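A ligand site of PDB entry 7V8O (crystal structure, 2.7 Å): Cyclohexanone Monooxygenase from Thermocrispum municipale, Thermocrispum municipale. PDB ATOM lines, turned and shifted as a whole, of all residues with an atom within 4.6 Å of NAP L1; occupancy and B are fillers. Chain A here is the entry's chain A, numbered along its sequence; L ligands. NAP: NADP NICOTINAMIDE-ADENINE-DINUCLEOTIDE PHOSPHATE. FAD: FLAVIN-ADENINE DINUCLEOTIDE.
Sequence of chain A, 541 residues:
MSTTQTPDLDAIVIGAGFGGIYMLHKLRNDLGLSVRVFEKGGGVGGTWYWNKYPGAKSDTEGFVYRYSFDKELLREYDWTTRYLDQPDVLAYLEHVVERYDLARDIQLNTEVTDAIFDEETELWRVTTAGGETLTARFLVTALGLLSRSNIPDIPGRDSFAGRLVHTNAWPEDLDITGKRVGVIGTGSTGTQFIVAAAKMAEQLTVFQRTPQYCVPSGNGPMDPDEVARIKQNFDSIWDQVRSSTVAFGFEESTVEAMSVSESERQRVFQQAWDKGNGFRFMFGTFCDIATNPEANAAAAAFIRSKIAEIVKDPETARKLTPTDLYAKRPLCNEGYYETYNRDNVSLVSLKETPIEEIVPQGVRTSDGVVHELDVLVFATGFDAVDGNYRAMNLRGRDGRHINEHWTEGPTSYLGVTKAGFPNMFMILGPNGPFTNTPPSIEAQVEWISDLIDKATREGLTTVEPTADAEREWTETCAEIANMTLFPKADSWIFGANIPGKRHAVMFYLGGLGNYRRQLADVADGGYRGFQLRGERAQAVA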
ATOM      1  N   ASP A  59      36.124 -11.999  15.005  1.00  0.00           N
ATOM      2  CA  ASP A  59      36.758 -13.350  15.062  1.00  0.00           C
ATOM      3  C   ASP A  59      38.127 -13.294  14.376  1.00  0.00           C
ATOM      4  O   ASP A  59      38.747 -14.354  14.263  1.00  0.00           O
ATOM      5  CB  ASP A  59      35.816 -14.445  14.533  1.00  0.00           C
ATOM      6  CG  ASP A  59      35.208 -14.238  13.150  1.00  0.00           C
ATOM      7  OD1 ASP A  59      35.485 -13.183  12.529  1.00  0.00           O
ATOM      8  OD2 ASP A  59      34.467 -15.141  12.687  1.00  0.00           O
ATOM      9  N   LEU A 146      28.128  -8.652   3.459  1.00  0.00           N
ATOM     10  CA  LEU A 146      27.200  -9.217   4.491  1.00  0.00           C
ATOM     11  C   LEU A 146      26.409  -8.090   5.164  1.00  0.00           C
ATOM     12  O   LEU A 146      26.550  -7.926   6.408  1.00  0.00           O
ATOM     13  CB  LEU A 146      28.043  -9.990   5.511  1.00  0.00           C
ATOM     14  CG  LEU A 146      28.950 -11.091   4.956  1.00  0.00           C
ATOM     15  CD1 LEU A 146      30.204 -11.218   5.795  1.00  0.00           C
ATOM     16  CD2 LEU A 146      28.220 -12.425   4.867  1.00  0.00           C
ATOM     17  N   ASN A 150      18.927 -11.794   5.360  1.00  0.00           N
ATOM     18  CA  ASN A 150      18.084 -12.901   4.844  1.00  0.00           C
ATOM     19  C   ASN A 150      17.145 -13.345   5.971  1.00  0.00           C
ATOM     20  O   ASN A 150      17.658 -13.865   6.986  1.00  0.00           O
ATOM     21  CB  ASN A 150      18.920 -14.085   4.361  1.00  0.00           C
ATOM     22  CG  ASN A 150      18.101 -15.339   4.137  1.00  0.00           C
ATOM     23  OD1 ASN A 150      17.159 -15.330   3.355  1.00  0.00           O
ATOM     24  ND2 ASN A 150      18.465 -16.422   4.815  1.00  0.00           N
ATOM     25  N   PRO A 152      14.186 -15.801   6.268  1.00  0.00           N
ATOM     26  CA  PRO A 152      13.406 -16.855   5.625  1.00  0.00           C
ATOM     27  C   PRO A 152      11.885 -16.767   5.869  1.00  0.00           C
ATOM     28  O   PRO A 152      11.497 -16.497   6.999  1.00  0.00           O
ATOM     29  CB  PRO A 152      13.946 -18.149   6.249  1.00  0.00           C
ATOM     30  CG  PRO A 152      15.365 -17.822   6.645  1.00  0.00           C
ATOM     31  CD  PRO A 152      15.358 -16.344   6.982  1.00  0.00           C
ATOM     32  N   ILE A 154       9.495 -18.511   6.830  1.00  0.00           N
ATOM     33  CA  ILE A 154       9.012 -19.664   7.654  1.00  0.00           C
ATOM     34  C   ILE A 154       7.512 -19.461   7.871  1.00  0.00           C
ATOM     35  O   ILE A 154       7.089 -18.370   8.248  1.00  0.00           O
ATOM     36  CB  ILE A 154       9.802 -19.782   8.978  1.00  0.00           C
ATOM     37  CG1 ILE A 154      11.232 -20.264   8.723  1.00  0.00           C
ATOM     38  CG2 ILE A 154       9.095 -20.684   9.982  1.00  0.00           C
ATOM     39  CD1 ILE A 154      12.126 -20.242   9.949  1.00  0.00           C
ATOM     40  N   ILE A 184      17.354 -19.029  15.747  1.00  0.00           N
ATOM     41  CA  ILE A 184      17.507 -19.923  14.552  1.00  0.00           C
ATOM     42  C   ILE A 184      18.822 -19.547  13.865  1.00  0.00           C
ATOM     43  O   ILE A 184      18.993 -18.361  13.527  1.00  0.00           O
ATOM     44  CB  ILE A 184      16.302 -19.799  13.588  1.00  0.00           C
ATOM     45  CG1 ILE A 184      14.988 -19.606  14.342  1.00  0.00           C
ATOM     46  CG2 ILE A 184      16.254 -21.000  12.661  1.00  0.00           C
ATOM     47  CD1 ILE A 184      13.780 -19.465  13.447  1.00  0.00           C
ATOM     48  N   GLY A 185      19.723 -20.515  13.701  1.00  0.00           N
ATOM     49  CA  GLY A 185      21.032 -20.318  13.052  1.00  0.00           C
ATOM     50  C   GLY A 185      22.191 -20.508  14.025  1.00  0.00           C
ATOM     51  O   GLY A 185      22.143 -19.941  15.127  1.00  0.00           O
ATOM     52  N   THR A 186      23.196 -21.256  13.606  1.00  0.00           N
ATOM     53  CA  THR A 186      24.391 -21.587  14.421  1.00  0.00           C
ATOM     54  C   THR A 186      25.643 -21.237  13.603  1.00  0.00           C
ATOM     55  O   THR A 186      26.607 -22.007  13.650  1.00  0.00           O
ATOM     56  CB  THR A 186      24.292 -23.044  14.891  1.00  0.00           C
ATOM     57  OG1 THR A 186      24.041 -23.880  13.763  1.00  0.00           O
ATOM     58  CG2 THR A 186      23.190 -23.237  15.901  1.00  0.00           C
ATOM     59  N   GLY A 187      25.601 -20.099  12.900  1.00  0.00           N
ATOM     60  CA  GLY A 187      26.778 -19.504  12.230  1.00  0.00           C
ATOM     61  C   GLY A 187      27.632 -18.693  13.202  1.00  0.00           C
ATOM     62  O   GLY A 187      27.385 -18.786  14.422  1.00  0.00           O
ATOM     63  N   SER A 188      28.613 -17.939  12.687  1.00  0.00           N
ATOM     64  CA  SER A 188      29.510 -17.049  13.475  1.00  0.00           C
ATOM     65  C   SER A 188      28.676 -16.161  14.399  1.00  0.00           C
ATOM     66  O   SER A 188      29.038 -16.026  15.601  1.00  0.00           O
ATOM     67  CB  SER A 188      30.391 -16.216  12.588  1.00  0.00           C
ATOM     68  OG  SER A 188      31.620 -16.870  12.328  1.00  0.00           O
ATOM     69  N   THR A 189      27.621 -15.574  13.844  1.00  0.00           N
ATOM     70  CA  THR A 189      26.696 -14.637  14.546  1.00  0.00           C
ATOM     71  C   THR A 189      25.883 -15.432  15.581  1.00  0.00           C
ATOM     72  O   THR A 189      25.922 -15.071  16.773  1.00  0.00           O
ATOM     73  CB  THR A 189      25.848 -13.893  13.515  1.00  0.00           C
ATOM     74  OG1 THR A 189      26.715 -13.001  12.827  1.00  0.00           O
ATOM     75  CG2 THR A 189      24.697 -13.136  14.134  1.00  0.00           C
ATOM     76  N   GLY A 190      25.198 -16.480  15.145  1.00  0.00           N
ATOM     77  CA  GLY A 190      24.340 -17.303  16.011  1.00  0.00           C
ATOM     78  C   GLY A 190      25.089 -17.766  17.245  1.00  0.00           C
ATOM     79  O   GLY A 190      24.571 -17.588  18.355  1.00  0.00           O
ATOM     80  N   ARG A 209      19.720 -26.085  12.391  1.00  0.00           N
ATOM     81  CA  ARG A 209      19.600 -26.981  11.209  1.00  0.00           C
ATOM     82  C   ARG A 209      20.936 -27.686  10.978  1.00  0.00           C
ATOM     83  O   ARG A 209      20.926 -28.928  10.844  1.00  0.00           O
ATOM     84  CB  ARG A 209      19.176 -26.204   9.956  1.00  0.00           C
ATOM     85  CG  ARG A 209      18.655 -27.110   8.847  1.00  0.00           C
ATOM     86  CD  ARG A 209      17.714 -26.368   7.901  1.00  0.00           C
ATOM     87  NE  ARG A 209      18.433 -25.345   7.168  1.00  0.00           N
ATOM     88  CZ  ARG A 209      17.880 -24.424   6.403  1.00  0.00           C
ATOM     89  NH1 ARG A 209      16.566 -24.370   6.253  1.00  0.00           N
ATOM     90  NH2 ARG A 209      18.653 -23.540   5.786  1.00  0.00           N
ATOM     91  N   THR A 210      22.036 -26.925  10.968  1.00  0.00           N
ATOM     92  CA  THR A 210      23.388 -27.421  10.578  1.00  0.00           C
ATOM     93  C   THR A 210      24.437 -27.011  11.605  1.00  0.00           C
ATOM     94  O   THR A 210      24.869 -25.862  11.648  1.00  0.00           O
ATOM     95  CB  THR A 210      23.745 -26.932   9.167  1.00  0.00           C
ATOM     96  OG1 THR A 210      22.626 -27.254   8.347  1.00  0.00           O
ATOM     97  CG2 THR A 210      25.001 -27.567   8.612  1.00  0.00           C
ATOM     98  N   GLN A 212      28.206 -26.534  13.050  1.00  0.00           N
ATOM     99  CA  GLN A 212      29.476 -26.166  12.377  1.00  0.00           C
ATOM    100  C   GLN A 212      30.656 -26.410  13.310  1.00  0.00           C
ATOM    101  O   GLN A 212      30.468 -26.467  14.541  1.00  0.00           O
ATOM    102  CB  GLN A 212      29.438 -24.707  11.931  1.00  0.00           C
ATOM    103  CG  GLN A 212      28.305 -24.421  10.962  1.00  0.00           C
ATOM    104  CD  GLN A 212      28.525 -23.134  10.192  1.00  0.00           C
ATOM    105  OE1 GLN A 212      29.645 -22.804   9.816  1.00  0.00           O
ATOM    106  NE2 GLN A 212      27.445 -22.415   9.951  1.00  0.00           N
ATOM    107  N   LYS A 328      33.116 -24.546   5.449  1.00  0.00           N
ATOM    108  CA  LYS A 328      32.464 -23.219   5.689  1.00  0.00           C
ATOM    109  C   LYS A 328      33.524 -22.278   6.267  1.00  0.00           C
ATOM    110  O   LYS A 328      34.634 -22.749   6.578  1.00  0.00           O
ATOM    111  CB  LYS A 328      31.257 -23.355   6.629  1.00  0.00           C
ATOM    112  CG  LYS A 328      30.281 -24.465   6.270  1.00  0.00           C
ATOM    113  CD  LYS A 328      28.987 -24.382   7.046  1.00  0.00           C
ATOM    114  CE  LYS A 328      27.892 -25.276   6.490  1.00  0.00           C
ATOM    115  NZ  LYS A 328      28.246 -26.715   6.612  1.00  0.00           N
ATOM    116  N   ARG A 329      33.213 -20.984   6.411  1.00  0.00           N
ATOM    117  CA  ARG A 329      34.157 -20.022   7.027  1.00  0.00           C
ATOM    118  C   ARG A 329      34.397 -20.451   8.469  1.00  0.00           C
ATOM    119  O   ARG A 329      33.438 -20.642   9.214  1.00  0.00           O
ATOM    120  CB  ARG A 329      33.648 -18.582   6.955  1.00  0.00           C
ATOM    121  CG  ARG A 329      34.657 -17.538   7.408  1.00  0.00           C
ATOM    122  CD  ARG A 329      34.052 -16.159   7.414  1.00  0.00           C
ATOM    123  NE  ARG A 329      35.048 -15.110   7.597  1.00  0.00           N
ATOM    124  CZ  ARG A 329      35.360 -14.537   8.755  1.00  0.00           C
ATOM    125  NH1 ARG A 329      36.283 -13.588   8.793  1.00  0.00           N
ATOM    126  NH2 ARG A 329      34.762 -14.910   9.881  1.00  0.00           N
ATOM    127  N   LEU A 350      16.878 -29.287  13.872  1.00  0.00           N
ATOM    128  CA  LEU A 350      15.837 -29.090  12.826  1.00  0.00           C
ATOM    129  C   LEU A 350      15.965 -30.182  11.755  1.00  0.00           C
ATOM    130  O   LEU A 350      14.993 -30.399  11.034  1.00  0.00           O
ATOM    131  CB  LEU A 350      15.987 -27.693  12.215  1.00  0.00           C
ATOM    132  CG  LEU A 350      15.838 -26.532  13.196  1.00  0.00           C
ATOM    133  CD1 LEU A 350      16.151 -25.200  12.532  1.00  0.00           C
ATOM    134  CD2 LEU A 350      14.449 -26.513  13.806  1.00  0.00           C
ATOM    135  N   ALA A 379      19.320 -15.591  13.430  1.00  0.00           N
ATOM    136  CA  ALA A 379      20.761 -15.553  13.100  1.00  0.00           C
ATOM    137  C   ALA A 379      20.962 -16.260  11.753  1.00  0.00           C
ATOM    138  O   ALA A 379      21.837 -17.151  11.666  1.00  0.00           O
ATOM    139  CB  ALA A 379      21.547 -16.217  14.216  1.00  0.00           C
ATOM    140  N   THR A 380      20.161 -15.872  10.754  1.00  0.00           N
ATOM    141  CA  THR A 380      19.981 -16.598   9.474  1.00  0.00           C
ATOM    142  C   THR A 380      20.800 -15.924   8.374  1.00  0.00           C
ATOM    143  O   THR A 380      20.542 -16.226   7.189  1.00  0.00           O
ATOM    144  CB  THR A 380      18.488 -16.740   9.144  1.00  0.00           C
ATOM    145  OG1 THR A 380      17.873 -15.448   9.211  1.00  0.00           O
ATOM    146  CG2 THR A 380      17.774 -17.691  10.076  1.00  0.00           C
ATOM    147  N   GLY A 381      21.754 -15.064   8.732  1.00  0.00           N
ATOM    148  CA  GLY A 381      22.778 -14.542   7.804  1.00  0.00           C
ATOM    149  C   GLY A 381      22.179 -13.662   6.721  1.00  0.00           C
ATOM    150  O   GLY A 381      21.110 -13.087   6.956  1.00  0.00           O
ATOM    151  N   PHE A 382      22.838 -13.593   5.558  1.00  0.00           N
ATOM    152  CA  PHE A 382      22.660 -12.521   4.539  1.00  0.00           C
ATOM    153  C   PHE A 382      22.532 -13.083   3.124  1.00  0.00           C
ATOM    154  O   PHE A 382      22.949 -14.224   2.853  1.00  0.00           O
ATOM    155  CB  PHE A 382      23.837 -11.555   4.582  1.00  0.00           C
ATOM    156  CG  PHE A 382      24.130 -10.984   5.943  1.00  0.00           C
ATOM    157  CD1 PHE A 382      24.853 -11.708   6.874  1.00  0.00           C
ATOM    158  CD2 PHE A 382      23.684  -9.716   6.292  1.00  0.00           C
ATOM    159  CE1 PHE A 382      25.125 -11.183   8.124  1.00  0.00           C
ATOM    160  CE2 PHE A 382      23.972  -9.186   7.540  1.00  0.00           C
ATOM    161  CZ  PHE A 382      24.679  -9.920   8.461  1.00  0.00           C
ATOM    162  N   SER A 491      27.240 -23.225   2.089  1.00  0.00           N
ATOM    163  CA  SER A 491      27.106 -22.047   2.993  1.00  0.00           C
ATOM    164  C   SER A 491      26.763 -20.825   2.138  1.00  0.00           C
ATOM    165  O   SER A 491      26.324 -21.034   0.997  1.00  0.00           O
ATOM    166  CB  SER A 491      28.366 -21.848   3.801  1.00  0.00           C
ATOM    167  OG  SER A 491      28.153 -20.864   4.808  1.00  0.00           O
ATOM    168  N   TRP A 492      26.974 -19.616   2.665  1.00  0.00           N
ATOM    169  CA  TRP A 492      26.604 -18.345   1.968  1.00  0.00           C
ATOM    170  C   TRP A 492      27.634 -17.994   0.874  1.00  0.00           C
ATOM    171  O   TRP A 492      27.323 -17.090   0.067  1.00  0.00           O
ATOM    172  CB  TRP A 492      26.432 -17.194   2.971  1.00  0.00           C
ATOM    173  CG  TRP A 492      27.648 -16.896   3.779  1.00  0.00           C
ATOM    174  CD1 TRP A 492      27.925 -17.344   5.042  1.00  0.00           C
ATOM    175  CD2 TRP A 492      28.781 -16.098   3.381  1.00  0.00           C
ATOM    176  NE1 TRP A 492      29.144 -16.874   5.453  1.00  0.00           N
ATOM    177  CE2 TRP A 492      29.693 -16.113   4.459  1.00  0.00           C
ATOM    178  CE3 TRP A 492      29.103 -15.380   2.229  1.00  0.00           C
ATOM    179  CZ2 TRP A 492      30.908 -15.433   4.405  1.00  0.00           C
ATOM    180  CZ3 TRP A 492      30.305 -14.719   2.176  1.00  0.00           C
ATOM    181  CH2 TRP A 492      31.188 -14.741   3.252  1.00  0.00           C
HETATM  182  PA  NAP L   1      25.495 -17.807   8.126  1.00  0.00           P
HETATM  183  O1A NAP L   1      26.904 -18.290   8.196  1.00  0.00           O
HETATM  184  O2A NAP L   1      24.847 -17.794   6.775  1.00  0.00           O
HETATM  185  O5B NAP L   1      24.603 -18.676   9.122  1.00  0.00           O
HETATM  186  C5B NAP L   1      23.163 -18.726   8.949  1.00  0.00           C
HETATM  187  C4B NAP L   1      22.600 -19.758   9.897  1.00  0.00           C
HETATM  188  O4B NAP L   1      21.156 -19.743   9.774  1.00  0.00           O
HETATM  189  C3B NAP L   1      23.027 -21.208   9.634  1.00  0.00           C
HETATM  190  O3B NAP L   1      23.133 -21.967  10.833  1.00  0.00           O
HETATM  191  C2B NAP L   1      21.888 -21.721   8.765  1.00  0.00           C
HETATM  192  O2B NAP L   1      21.783 -23.148   8.831  1.00  0.00           O
HETATM  193  C1B NAP L   1      20.702 -21.035   9.439  1.00  0.00           C
HETATM  194  N9A NAP L   1      19.531 -20.902   8.568  1.00  0.00           N
HETATM  195  C8A NAP L   1      19.462 -20.211   7.387  1.00  0.00           C
HETATM  196  N7A NAP L   1      18.286 -20.286   6.813  1.00  0.00           N
HETATM  197  C5A NAP L   1      17.535 -21.079   7.674  1.00  0.00           C
HETATM  198  C6A NAP L   1      16.204 -21.529   7.623  1.00  0.00           C
HETATM  199  N6A NAP L   1      15.366 -21.228   6.642  1.00  0.00           N
HETATM  200  N1A NAP L   1      15.770 -22.308   8.647  1.00  0.00           N
HETATM  201  C2A NAP L   1      16.626 -22.598   9.639  1.00  0.00           C
HETATM  202  N3A NAP L   1      17.891 -22.234   9.784  1.00  0.00           N
HETATM  203  C4A NAP L   1      18.296 -21.462   8.758  1.00  0.00           C
HETATM  204  O3  NAP L   1      25.361 -16.320   8.737  1.00  0.00           O
HETATM  205  PN  NAP L   1      25.994 -15.501   9.968  1.00  0.00           P
HETATM  206  O1N NAP L   1      25.387 -14.137  10.058  1.00  0.00           O
HETATM  207  O2N NAP L   1      25.894 -16.378  11.186  1.00  0.00           O
HETATM  208  O5D NAP L   1      27.536 -15.381   9.534  1.00  0.00           O
HETATM  209  C5D NAP L   1      28.002 -14.682   8.334  1.00  0.00           C
HETATM  210  C4D NAP L   1      29.223 -13.840   8.649  1.00  0.00           C
HETATM  211  O4D NAP L   1      28.934 -13.029   9.812  1.00  0.00           O
HETATM  212  C3D NAP L   1      30.536 -14.590   8.963  1.00  0.00           C
HETATM  213  O3D NAP L   1      31.378 -14.660   7.822  1.00  0.00           O
HETATM  214  C2D NAP L   1      31.202 -13.762  10.064  1.00  0.00           C
HETATM  215  O2D NAP L   1      32.342 -13.043   9.614  1.00  0.00           O
HETATM  216  C1D NAP L   1      30.117 -12.813  10.573  1.00  0.00           C
HETATM  217  N1N NAP L   1      29.785 -13.035  12.023  1.00  0.00           N
HETATM  218  P2B NAP L   1      22.119 -23.843   7.407  1.00  0.00           P
HETATM  219  O1X NAP L   1      21.299 -25.113   7.367  1.00  0.00           O
HETATM  220  O2X NAP L   1      21.698 -22.857   6.335  1.00  0.00           O
HETATM  221  O3X NAP L   1      23.612 -24.123   7.378  1.00  0.00           O
HETATM  222  PA  FAD L   2      29.594  -3.092   5.744  1.00  0.00           P
HETATM  223  O1A FAD L   2      30.293  -2.776   7.029  1.00  0.00           O
HETATM  224  O2A FAD L   2      28.487  -4.104   5.739  1.00  0.00           O
HETATM  225  O5B FAD L   2      29.039  -1.713   5.116  1.00  0.00           O
HETATM  226  C5B FAD L   2      28.037  -1.717   4.052  1.00  0.00           C
HETATM  227  C4B FAD L   2      27.101  -0.551   4.258  1.00  0.00           C
HETATM  228  O4B FAD L   2      26.454  -0.218   2.994  1.00  0.00           O
HETATM  229  C3B FAD L   2      25.959  -0.786   5.273  1.00  0.00           C
HETATM  230  O3B FAD L   2      25.939   0.228   6.276  1.00  0.00           O
HETATM  231  C2B FAD L   2      24.692  -0.761   4.401  1.00  0.00           C
HETATM  232  O2B FAD L   2      23.565  -0.287   5.107  1.00  0.00           O
HETATM  233  C1B FAD L   2      25.133   0.158   3.263  1.00  0.00           C
HETATM  234  N9A FAD L   2      24.333   0.024   2.055  1.00  0.00           N
HETATM  235  C8A FAD L   2      24.047  -1.143   1.377  1.00  0.00           C
HETATM  236  N7A FAD L   2      23.265  -0.938   0.347  1.00  0.00           N
HETATM  237  C5A FAD L   2      23.008   0.431   0.355  1.00  0.00           C
HETATM  238  C6A FAD L   2      22.244   1.269  -0.483  1.00  0.00           C
HETATM  239  N6A FAD L   2      21.557   0.812  -1.524  1.00  0.00           N
HETATM  240  N1A FAD L   2      22.206   2.582  -0.182  1.00  0.00           N
HETATM  241  C2A FAD L   2      22.885   3.018   0.884  1.00  0.00           C
HETATM  242  N3A FAD L   2      23.637   2.330   1.737  1.00  0.00           N
HETATM  243  C4A FAD L   2      23.662   1.026   1.410  1.00  0.00           C
HETATM  244  N1  FAD L   2      30.280  -9.246  10.319  1.00  0.00           N
HETATM  245  C2  FAD L   2      29.296  -9.284  11.262  1.00  0.00           C
HETATM  246  O2  FAD L   2      28.119  -9.093  10.960  1.00  0.00           O
HETATM  247  N3  FAD L   2      29.572  -9.534  12.579  1.00  0.00           N
HETATM  248  C4  FAD L   2      30.844  -9.760  13.020  1.00  0.00           C
HETATM  249  O4  FAD L   2      31.042  -9.986  14.202  1.00  0.00           O
HETATM  250  C4X FAD L   2      31.892  -9.739  12.064  1.00  0.00           C
HETATM  251  N5  FAD L   2      33.116  -9.956  12.467  1.00  0.00           N
HETATM  252  C5X FAD L   2      34.107  -9.960  11.526  1.00  0.00           C
HETATM  253  C6  FAD L   2      35.413 -10.216  11.939  1.00  0.00           C
HETATM  254  C7  FAD L   2      36.434 -10.255  11.033  1.00  0.00           C
HETATM  255  C7M FAD L   2      37.822 -10.531  11.518  1.00  0.00           C
HETATM  256  C8  FAD L   2      36.191 -10.026   9.669  1.00  0.00           C
HETATM  257  C8M FAD L   2      37.322 -10.073   8.682  1.00  0.00           C
HETATM  258  C9  FAD L   2      34.935  -9.733   9.252  1.00  0.00           C
HETATM  259  C9A FAD L   2      33.869  -9.707  10.158  1.00  0.00           C
HETATM  260  N10 FAD L   2      32.559  -9.469   9.761  1.00  0.00           N
HETATM  261  C10 FAD L   2      31.527  -9.475  10.694  1.00  0.00           C
HETATM  262  C1' FAD L   2      32.287  -9.135   8.346  1.00  0.00           C
HETATM  263  C2' FAD L   2      32.296  -7.611   8.169  1.00  0.00           C
HETATM  264  O2' FAD L   2      31.157  -7.272   7.401  1.00  0.00           O
HETATM  265  C3' FAD L   2      33.554  -7.009   7.545  1.00  0.00           C
HETATM  266  O3' FAD L   2      34.698  -7.319   8.323  1.00  0.00           O
HETATM  267  C4' FAD L   2      33.536  -5.482   7.391  1.00  0.00           C
HETATM  268  O4' FAD L   2      33.195  -4.870   8.635  1.00  0.00           O
HETATM  269  C5' FAD L   2      32.550  -5.003   6.345  1.00  0.00           C
HETATM  270  O5' FAD L   2      32.822  -3.621   5.977  1.00  0.00           O
HETATM  271  P   FAD L   2      32.269  -3.062   4.580  1.00  0.00           P
HETATM  272  O1P FAD L   2      32.447  -1.585   4.557  1.00  0.00           O
HETATM  273  O2P FAD L   2      32.895  -3.902   3.520  1.00  0.00           O
HETATM  274  O3P FAD L   2      30.719  -3.483   4.673  1.00  0.00           O
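O of Ala 379 sits close to O4B of NAP L1 (3.3 Å). Merely in contact with NAP L1: Gly 381 (3.3 Å), Gly 185 (3.3 Å), Thr 380 (3.4 Å), Pro 152 (3.4 Å), Gly 187 (3.4 Å), Ile 184 (3.4 Å), Trp 492 (3.4 Å), Phe 382 (3.5 Å), Leu 350 (3.9 Å) and Leu 146 (3.998 Å). Hydrophobic or aromatic side chains within 4 Å of NAP L1: Leu 146, Pro 152, Ile 184, Leu 350, Phe 382 and Trp 492. Within 4 Å of NAP L1: Leu 146, Pro 152, Ile 184, Gly 185, Thr 186, Gly 187, Ser 188, Thr 189, Arg 209, Thr 210, Arg 329, Leu 350, Ala 379, Thr 380, Gly 381, Phe 382 and Trp 492.
The backbone carbonyl oxygen of Thr 210 sits at hydrogen-bond distance from the side-chain hydroxyl of Thr 186 (3.0 Å). The side-chain carboxylate (OD2) of Asp 59 is in salt-bridge range of the guanidinium group (NH2) of Arg 329 (2.8 Å). The backbone NH (N) of Ala 379 lies within hydrogen-bond range of the backbone carbonyl oxygen (O) of Ile 184 (2.8 Å). N of Asn 150 lies within hydrogen-bond range of O of Gly 381. OD2 of Asp 59 is in hydrogen-bond range of OG of Ser 188 (3.4 Å). OG1 of Thr 380 sits at hydrogen-bond distance from O of Asn 150 (2.7 Å).
The side-chain hydroxyl (OG1) of Thr 210 lies within hydrogen-bond range of an oxygen (O1X) of NAP L1 (2.7 Å). O3B of NAP L1 sits at hydrogen-bond distance from N of Thr 186, at 2.9 Å. The guanidinium group (NE) of Arg 209 lies within salt-bridge range of an oxygen (O1X) of NAP L1. The guanidinium group (NH2) of Arg 329 sits at hydrogen-bond distance from an oxygen (O2D) of NAP L1 (3.1 Å). The backbone NH (N) of Thr 189 is in hydrogen-bond range of an oxygen (O2N) of NAP L1. The side-chain hydroxyl (OG1) of Thr 189 sits at hydrogen-bond distance from a nitrogen (N1N) of NAP L1 (3.2 Å). The backbone NH of Ser 188 is in hydrogen-bond range of an oxygen (O2N) of NAP L1.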
